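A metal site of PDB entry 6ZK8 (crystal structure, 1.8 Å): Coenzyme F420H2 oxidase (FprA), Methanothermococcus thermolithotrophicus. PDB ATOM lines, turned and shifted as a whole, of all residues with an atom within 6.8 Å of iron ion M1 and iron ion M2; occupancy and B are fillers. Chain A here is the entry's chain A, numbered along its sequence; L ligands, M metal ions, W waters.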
ATOM      1  N   TYR A  25     -16.290  -1.842  33.730  1.00  0.00           N
ATOM      2  CA  TYR A  25     -15.863  -2.265  32.398  1.00  0.00           C
ATOM      3  C   TYR A  25     -16.706  -3.483  32.049  1.00  0.00           C
ATOM      4  O   TYR A  25     -17.039  -4.282  32.932  1.00  0.00           O
ATOM      5  CB  TYR A  25     -14.373  -2.610  32.378  1.00  0.00           C
ATOM      6  CG  TYR A  25     -13.748  -2.659  30.999  1.00  0.00           C
ATOM      7  CD1 TYR A  25     -13.719  -1.541  30.203  1.00  0.00           C
ATOM      8  CD2 TYR A  25     -13.180  -3.829  30.498  1.00  0.00           C
ATOM      9  CE1 TYR A  25     -13.149  -1.570  28.941  1.00  0.00           C
ATOM     10  CE2 TYR A  25     -12.582  -3.855  29.232  1.00  0.00           C
ATOM     11  CZ  TYR A  25     -12.575  -2.703  28.464  1.00  0.00           C
ATOM     12  OH  TYR A  25     -12.017  -2.693  27.200  1.00  0.00           O
ATOM     13  N   HIS A  26     -17.017  -3.650  30.757  1.00  0.00           N
ATOM     14  CA  HIS A  26     -17.900  -4.734  30.263  1.00  0.00           C
ATOM     15  C   HIS A  26     -19.188  -4.585  31.060  1.00  0.00           C
ATOM     16  O   HIS A  26     -19.708  -3.461  31.164  1.00  0.00           O
ATOM     17  CB  HIS A  26     -17.224  -6.086  30.416  1.00  0.00           C
ATOM     18  CG  HIS A  26     -15.960  -6.259  29.633  1.00  0.00           C
ATOM     19  ND1 HIS A  26     -14.939  -7.090  30.068  1.00  0.00           N
ATOM     20  CD2 HIS A  26     -15.557  -5.759  28.443  1.00  0.00           C
ATOM     21  CE1 HIS A  26     -13.975  -7.099  29.160  1.00  0.00           C
ATOM     22  NE2 HIS A  26     -14.314  -6.283  28.175  1.00  0.00           N
ATOM     23  N   TYR A  28     -19.173  -5.247  34.475  1.00  0.00           N
ATOM     24  CA  TYR A  28     -18.722  -5.577  35.809  1.00  0.00           C
ATOM     25  C   TYR A  28     -17.997  -4.419  36.453  1.00  0.00           C
ATOM     26  O   TYR A  28     -17.646  -3.410  35.849  1.00  0.00           O
ATOM     27  CB  TYR A  28     -17.857  -6.855  35.869  1.00  0.00           C
ATOM     28  CG  TYR A  28     -16.701  -6.887  34.914  1.00  0.00           C
ATOM     29  CD1 TYR A  28     -15.636  -6.055  35.071  1.00  0.00           C
ATOM     30  CD2 TYR A  28     -16.682  -7.774  33.845  1.00  0.00           C
ATOM     31  CE1 TYR A  28     -14.592  -6.074  34.160  1.00  0.00           C
ATOM     32  CE2 TYR A  28     -15.617  -7.825  32.956  1.00  0.00           C
ATOM     33  CZ  TYR A  28     -14.589  -6.969  33.128  1.00  0.00           C
ATOM     34  OH  TYR A  28     -13.528  -6.990  32.243  1.00  0.00           O
ATOM     35  N   TYR A  35      -3.518  -3.163  32.267  1.00  0.00           N
ATOM     36  CA  TYR A  35      -3.443  -3.629  30.880  1.00  0.00           C
ATOM     37  C   TYR A  35      -1.987  -4.085  30.744  1.00  0.00           C
ATOM     38  O   TYR A  35      -1.094  -3.251  30.571  1.00  0.00           O
ATOM     39  CB  TYR A  35      -3.841  -2.542  29.867  1.00  0.00           C
ATOM     40  CG  TYR A  35      -5.142  -1.881  30.287  1.00  0.00           C
ATOM     41  CD1 TYR A  35      -6.306  -2.616  30.396  1.00  0.00           C
ATOM     42  CD2 TYR A  35      -5.197  -0.542  30.637  1.00  0.00           C
ATOM     43  CE1 TYR A  35      -7.476  -2.038  30.862  1.00  0.00           C
ATOM     44  CE2 TYR A  35      -6.353   0.045  31.051  1.00  0.00           C
ATOM     45  CZ  TYR A  35      -7.485  -0.698  31.171  1.00  0.00           C
ATOM     46  OH  TYR A  35      -8.626  -0.144  31.616  1.00  0.00           O
ATOM     47  N   HIS A  84      -5.140 -10.330  20.696  1.00  0.00           N
ATOM     48  CA  HIS A  84      -6.553 -10.108  20.958  1.00  0.00           C
ATOM     49  C   HIS A  84      -6.862  -8.713  20.471  1.00  0.00           C
ATOM     50  O   HIS A  84      -6.066  -7.798  20.691  1.00  0.00           O
ATOM     51  CB  HIS A  84      -6.824 -10.308  22.459  1.00  0.00           C
ATOM     52  CG  HIS A  84      -8.240 -10.087  22.886  1.00  0.00           C
ATOM     53  ND1 HIS A  84      -9.315 -10.381  22.074  1.00  0.00           N
ATOM     54  CD2 HIS A  84      -8.766  -9.645  24.054  1.00  0.00           C
ATOM     55  CE1 HIS A  84     -10.443 -10.104  22.716  1.00  0.00           C
ATOM     56  NE2 HIS A  84     -10.133  -9.663  23.925  1.00  0.00           N
ATOM     57  N   GLU A  86      -9.656  -6.762  21.138  1.00  0.00           N
ATOM     58  CA  GLU A  86     -10.402  -5.852  22.012  1.00  0.00           C
ATOM     59  C   GLU A  86      -9.518  -4.693  22.471  1.00  0.00           C
ATOM     60  O   GLU A  86      -8.344  -4.880  22.766  1.00  0.00           O
ATOM     61  CB  GLU A  86     -10.970  -6.617  23.221  1.00  0.00           C
ATOM     62  CG  GLU A  86     -11.942  -5.803  24.012  1.00  0.00           C
ATOM     63  CD  GLU A  86     -12.861  -6.582  24.940  1.00  0.00           C
ATOM     64  OE1 GLU A  86     -13.792  -5.948  25.504  1.00  0.00           O
ATOM     65  OE2 GLU A  86     -12.689  -7.808  25.082  1.00  0.00           O
ATOM     66  N   LYS A  87     -10.099  -3.502  22.554  1.00  0.00           N
ATOM     67  CA  LYS A  87      -9.284  -2.303  22.553  1.00  0.00           C
ATOM     68  C   LYS A  87      -8.564  -2.053  23.876  1.00  0.00           C
ATOM     69  O   LYS A  87      -7.682  -1.185  23.908  1.00  0.00           O
ATOM     70  CB  LYS A  87     -10.140  -1.094  22.162  1.00  0.00           C
ATOM     71  CG  LYS A  87     -11.234  -0.685  23.079  1.00  0.00           C
ATOM     72  CD  LYS A  87     -12.204   0.255  22.307  1.00  0.00           C
ATOM     73  CE  LYS A  87     -12.534   1.503  23.053  1.00  0.00           C
ATOM     74  NZ  LYS A  87     -13.198   2.507  22.135  1.00  0.00           N
ATOM     75  N   ASP A  88      -8.872  -2.781  24.950  1.00  0.00           N
ATOM     76  CA  ASP A  88      -8.027  -2.611  26.135  1.00  0.00           C
ATOM     77  C   ASP A  88      -6.675  -3.288  25.973  1.00  0.00           C
ATOM     78  O   ASP A  88      -5.792  -3.142  26.820  1.00  0.00           O
ATOM     79  CB  ASP A  88      -8.754  -3.088  27.410  1.00  0.00           C
ATOM     80  CG  ASP A  88      -9.281  -4.503  27.294  1.00  0.00           C
ATOM     81  OD1 ASP A  88      -9.919  -4.836  26.303  1.00  0.00           O
ATOM     82  OD2 ASP A  88      -9.037  -5.283  28.238  1.00  0.00           O
ATOM     83  N   HIS A  89      -6.479  -4.010  24.872  1.00  0.00           N
ATOM     84  CA  HIS A  89      -5.184  -4.636  24.572  1.00  0.00           C
ATOM     85  C   HIS A  89      -4.616  -4.218  23.223  1.00  0.00           C
ATOM     86  O   HIS A  89      -3.457  -4.548  22.944  1.00  0.00           O
ATOM     87  CB  HIS A  89      -5.304  -6.169  24.637  1.00  0.00           C
ATOM     88  CG  HIS A  89      -5.961  -6.655  25.888  1.00  0.00           C
ATOM     89  ND1 HIS A  89      -5.398  -6.464  27.138  1.00  0.00           N
ATOM     90  CD2 HIS A  89      -7.159  -7.245  26.105  1.00  0.00           C
ATOM     91  CE1 HIS A  89      -6.231  -6.909  28.064  1.00  0.00           C
ATOM     92  NE2 HIS A  89      -7.318  -7.383  27.463  1.00  0.00           N
ATOM     93  N   HIS A 152     -11.316 -15.041  24.800  1.00  0.00           N
ATOM     94  CA  HIS A 152     -12.769 -15.064  24.795  1.00  0.00           C
ATOM     95  C   HIS A 152     -13.453 -14.458  23.556  1.00  0.00           C
ATOM     96  O   HIS A 152     -14.686 -14.312  23.530  1.00  0.00           O
ATOM     97  CB  HIS A 152     -13.323 -14.322  26.057  1.00  0.00           C
ATOM     98  CG  HIS A 152     -13.086 -12.822  26.038  1.00  0.00           C
ATOM     99  ND1 HIS A 152     -14.081 -11.901  26.278  1.00  0.00           N
ATOM    100  CD2 HIS A 152     -11.953 -12.108  25.823  1.00  0.00           C
ATOM    101  CE1 HIS A 152     -13.580 -10.676  26.189  1.00  0.00           C
ATOM    102  NE2 HIS A 152     -12.285 -10.777  25.912  1.00  0.00           N
ATOM    103  N   TRP A 153     -12.660 -14.091  22.569  1.00  0.00           N
ATOM    104  CA  TRP A 153     -13.152 -13.621  21.284  1.00  0.00           C
ATOM    105  C   TRP A 153     -12.668 -14.540  20.162  1.00  0.00           C
ATOM    106  O   TRP A 153     -11.712 -15.315  20.338  1.00  0.00           O
ATOM    107  CB  TRP A 153     -12.686 -12.182  20.994  1.00  0.00           C
ATOM    108  CG  TRP A 153     -13.523 -11.107  21.690  1.00  0.00           C
ATOM    109  CD1 TRP A 153     -14.392 -11.286  22.722  1.00  0.00           C
ATOM    110  CD2 TRP A 153     -13.525  -9.719  21.379  1.00  0.00           C
ATOM    111  NE1 TRP A 153     -14.944 -10.076  23.090  1.00  0.00           N
ATOM    112  CE2 TRP A 153     -14.426  -9.093  22.276  1.00  0.00           C
ATOM    113  CE3 TRP A 153     -12.861  -8.926  20.434  1.00  0.00           C
ATOM    114  CZ2 TRP A 153     -14.675  -7.720  22.260  1.00  0.00           C
ATOM    115  CZ3 TRP A 153     -13.118  -7.553  20.411  1.00  0.00           C
ATOM    116  CH2 TRP A 153     -14.019  -6.969  21.325  1.00  0.00           C
ATOM    117  N   SER A 156      -8.843 -14.474  19.480  1.00  0.00           N
ATOM    118  CA  SER A 156      -7.898 -14.606  20.575  1.00  0.00           C
ATOM    119  C   SER A 156      -6.829 -15.653  20.277  1.00  0.00           C
ATOM    120  O   SER A 156      -7.041 -16.630  19.549  1.00  0.00           O
ATOM    121  CB  SER A 156      -8.633 -14.944  21.874  1.00  0.00           C
ATOM    122  OG  SER A 156      -9.546 -13.929  22.250  1.00  0.00           O
ATOM    123  N   ASN A 170      -3.190 -13.525  27.296  1.00  0.00           N
ATOM    124  CA  ASN A 170      -4.126 -12.395  27.136  1.00  0.00           C
ATOM    125  C   ASN A 170      -5.192 -12.501  28.222  1.00  0.00           C
ATOM    126  O   ASN A 170      -4.809 -12.674  29.381  1.00  0.00           O
ATOM    127  CB  ASN A 170      -4.649 -12.365  25.705  1.00  0.00           C
ATOM    128  CG  ASN A 170      -5.366 -11.067  25.379  1.00  0.00           C
ATOM    129  OD1 ASN A 170      -6.604 -10.983  25.439  1.00  0.00           O
ATOM    130  ND2 ASN A 170      -4.580 -10.033  25.047  1.00  0.00           N
ATOM    131  N   ASP A 171      -6.479 -12.414  27.894  1.00  0.00           N
ATOM    132  CA  ASP A 171      -7.484 -12.296  28.947  1.00  0.00           C
ATOM    133  C   ASP A 171      -7.554 -13.549  29.812  1.00  0.00           C
ATOM    134  O   ASP A 171      -7.837 -13.459  31.017  1.00  0.00           O
ATOM    135  CB  ASP A 171      -8.874 -12.015  28.360  1.00  0.00           C
ATOM    136  CG  ASP A 171      -9.087 -10.553  27.912  1.00  0.00           C
ATOM    137  OD1 ASP A 171      -8.814  -9.591  28.660  1.00  0.00           O
ATOM    138  OD2 ASP A 171      -9.556 -10.362  26.779  1.00  0.00           O
ATOM    139  N   HIS A 176      -8.980  -8.694  37.496  1.00  0.00           N
ATOM    140  CA  HIS A 176      -9.020  -7.241  37.520  1.00  0.00           C
ATOM    141  C   HIS A 176      -8.553  -6.780  38.870  1.00  0.00           C
ATOM    142  O   HIS A 176      -9.342  -6.611  39.795  1.00  0.00           O
ATOM    143  CB  HIS A 176     -10.413  -6.728  37.175  1.00  0.00           C
ATOM    144  CG  HIS A 176     -10.729  -6.825  35.726  1.00  0.00           C
ATOM    145  ND1 HIS A 176      -9.859  -6.370  34.753  1.00  0.00           N
ATOM    146  CD2 HIS A 176     -11.786  -7.350  35.072  1.00  0.00           C
ATOM    147  CE1 HIS A 176     -10.381  -6.594  33.566  1.00  0.00           C
ATOM    148  NE2 HIS A 176     -11.555  -7.196  33.735  1.00  0.00           N
ATOM    149  N   PHE A 199     -13.519 -12.918  37.606  1.00  0.00           N
ATOM    150  CA  PHE A 199     -13.184 -12.864  36.188  1.00  0.00           C
ATOM    151  C   PHE A 199     -13.758 -14.062  35.435  1.00  0.00           C
ATOM    152  O   PHE A 199     -14.454 -13.893  34.428  1.00  0.00           O
ATOM    153  CB  PHE A 199     -11.656 -12.806  36.065  1.00  0.00           C
ATOM    154  CG  PHE A 199     -11.157 -12.347  34.722  1.00  0.00           C
ATOM    155  CD1 PHE A 199     -11.006 -13.233  33.680  1.00  0.00           C
ATOM    156  CD2 PHE A 199     -10.809 -11.034  34.519  1.00  0.00           C
ATOM    157  CE1 PHE A 199     -10.559 -12.824  32.453  1.00  0.00           C
ATOM    158  CE2 PHE A 199     -10.347 -10.625  33.304  1.00  0.00           C
ATOM    159  CZ  PHE A 199     -10.200 -11.523  32.268  1.00  0.00           C
ATOM    160  N   LEU A 203     -16.732 -13.614  32.645  1.00  0.00           N
ATOM    161  CA  LEU A 203     -16.201 -13.646  31.286  1.00  0.00           C
ATOM    162  C   LEU A 203     -16.000 -15.030  30.705  1.00  0.00           C
ATOM    163  O   LEU A 203     -16.057 -15.176  29.477  1.00  0.00           O
ATOM    164  CB  LEU A 203     -14.862 -12.897  31.228  1.00  0.00           C
ATOM    165  CG  LEU A 203     -14.953 -11.407  31.478  1.00  0.00           C
ATOM    166  CD1 LEU A 203     -13.600 -10.763  31.693  1.00  0.00           C
ATOM    167  CD2 LEU A 203     -15.667 -10.733  30.307  1.00  0.00           C
ATOM    168  N   SER A 233      -3.179 -10.671  30.575  1.00  0.00           N
ATOM    169  CA  SER A 233      -3.302  -9.273  30.159  1.00  0.00           C
ATOM    170  C   SER A 233      -3.991  -8.388  31.202  1.00  0.00           C
ATOM    171  O   SER A 233      -4.089  -7.184  30.983  1.00  0.00           O
ATOM    172  CB  SER A 233      -4.057  -9.201  28.825  1.00  0.00           C
ATOM    173  OG  SER A 233      -5.396  -9.620  29.006  1.00  0.00           O
ATOM    174  N   HIS A 234      -4.450  -8.956  32.320  1.00  0.00           N
ATOM    175  CA  HIS A 234      -5.013  -8.174  33.415  1.00  0.00           C
ATOM    176  C   HIS A 234      -4.530  -8.780  34.714  1.00  0.00           C
ATOM    177  O   HIS A 234      -4.563 -10.003  34.890  1.00  0.00           O
ATOM    178  CB  HIS A 234      -6.559  -8.180  33.431  1.00  0.00           C
ATOM    179  CG  HIS A 234      -7.196  -7.582  32.214  1.00  0.00           C
ATOM    180  ND1 HIS A 234      -7.230  -6.219  31.991  1.00  0.00           N
ATOM    181  CD2 HIS A 234      -7.825  -8.151  31.166  1.00  0.00           C
ATOM    182  CE1 HIS A 234      -7.834  -5.982  30.851  1.00  0.00           C
ATOM    183  NE2 HIS A 234      -8.217  -7.136  30.324  1.00  0.00           N
HETATM  184  N1  LIG L   1     -19.823 -10.094  19.777  1.00  0.00           N
HETATM  185  C1  LIG L   1     -20.588 -11.078  19.165  1.00  0.00           C
HETATM  186  O1  LIG L   1     -20.910 -10.947  17.993  1.00  0.00           O
HETATM  187  N2  LIG L   1     -20.984 -12.206  19.875  1.00  0.00           N
HETATM  188  C2  LIG L   1     -20.610 -12.340  21.191  1.00  0.00           C
HETATM  189  O2  LIG L   1     -20.960 -13.332  21.825  1.00  0.00           O
HETATM  190  C3  LIG L   1     -19.837 -11.356  21.809  1.00  0.00           C
HETATM  191  N3  LIG L   1     -19.455 -11.507  23.114  1.00  0.00           N
HETATM  192  C4  LIG L   1     -18.729 -10.497  23.727  1.00  0.00           C
HETATM  193  C5  LIG L   1     -18.384 -10.615  25.062  1.00  0.00           C
HETATM  194  C6  LIG L   1     -17.640  -9.625  25.684  1.00  0.00           C
HETATM  195  C7  LIG L   1     -17.265  -9.774  27.127  1.00  0.00           C
HETATM  196  C8  LIG L   1     -17.267  -8.488  24.970  1.00  0.00           C
HETATM  197  C9  LIG L   1     -16.470  -7.418  25.652  1.00  0.00           C
HETATM  198  C10 LIG L   1     -17.620  -8.370  23.629  1.00  0.00           C
HETATM  199  C11 LIG L   1     -18.349  -9.368  23.004  1.00  0.00           C
HETATM  200  N4  LIG L   1     -18.722  -9.253  21.672  1.00  0.00           N
HETATM  201  C12 LIG L   1     -19.455 -10.247  21.084  1.00  0.00           C
HETATM  202  C13 LIG L   1     -18.316  -8.087  20.835  1.00  0.00           C
HETATM  203  C14 LIG L   1     -19.130  -6.818  20.969  1.00  0.00           C
HETATM  204  O3  LIG L   1     -20.462  -6.993  20.510  1.00  0.00           O
HETATM  205  C15 LIG L   1     -18.426  -5.810  20.050  1.00  0.00           C
HETATM  206  O4  LIG L   1     -17.197  -5.450  20.636  1.00  0.00           O
HETATM  207  C16 LIG L   1     -19.273  -4.574  19.776  1.00  0.00           C
HETATM  208  O5  LIG L   1     -18.715  -3.820  18.724  1.00  0.00           O
HETATM  209  C17 LIG L   1     -19.332  -3.715  21.041  1.00  0.00           C
HETATM  210  O6  LIG L   1     -20.212  -2.649  20.794  1.00  0.00           O
HETATM  211  P1  LIG L   1     -20.182  -1.363  21.730  1.00  0.00           P
HETATM  212  O7  LIG L   1     -20.013  -1.835  23.133  1.00  0.00           O
HETATM  213  O8  LIG L   1     -19.004  -0.531  21.343  1.00  0.00           O
HETATM  214  O9  LIG L   1     -21.454  -0.577  21.501  1.00  0.00           O
HETATM  215 FE    FE M   1      -9.103  -7.605  28.330  1.00  0.00          FE
HETATM  216 FE    FE M   2     -11.024  -9.003  26.014  1.00  0.00          FE
HETATM  217  O   HOH W   1     -10.530  -7.599  27.071  1.00  0.00           O
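The side-chain amide oxygen (OD1) of Asn 170 sits close to the side-chain carboxylate (OD2) of Asp 171 (3.3 Å). The backbone NH (N) of His 152 lies within hydrogen-bond range of the side-chain hydroxyl (OG) of Ser 156, at 3.3 Å. OE1 of Glu 86 is in hydrogen-bond range of NE2 of His 26. OH of Tyr 25 lies within hydrogen-bond range of OD1 of Asp 88 (3.1 Å). The side-chain hydroxyl of Ser 233 sits close to a ring nitrogen (NE2) of His 89, 3.3 Å away. The backbone NH (N) of Asp 171 sits at hydrogen-bond distance from the side-chain hydroxyl (OG) of Ser 233, at 3.2 Å.
The nearest printed residue that does not touch iron ion M2 is His 89 (4.2 Å).
Within 4 Å of iron ion M1: Asp 88, His 89, Asp 171 and His 234.
Water W1 is bound to iron ion M1. Iron ion M1 is bound by NE2 of His 89 (2.0 Å). Iron ion M1 is bound by OD1 of Asp 171, 2.0 Å away. NE2 of His 234 binds iron ion M1 (2.2 Å). Iron ion M1 is bound by OD2 of Asp 88. Iron ion M1 has five donor atoms within binding distance.
Water W1 binds iron ion M2 (1.8 Å). The side-chain carboxylate (OD2) of Asp 171 binds iron ion M2 (2.1 Å). NE2 of His 152 is bound to iron ion M2, at 2.2 Å. OE2 of Glu 86 is bound to iron ion M2 (2.3 Å). A ring nitrogen (NE2) of His 84 is bound to iron ion M2, at 2.4 Å.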
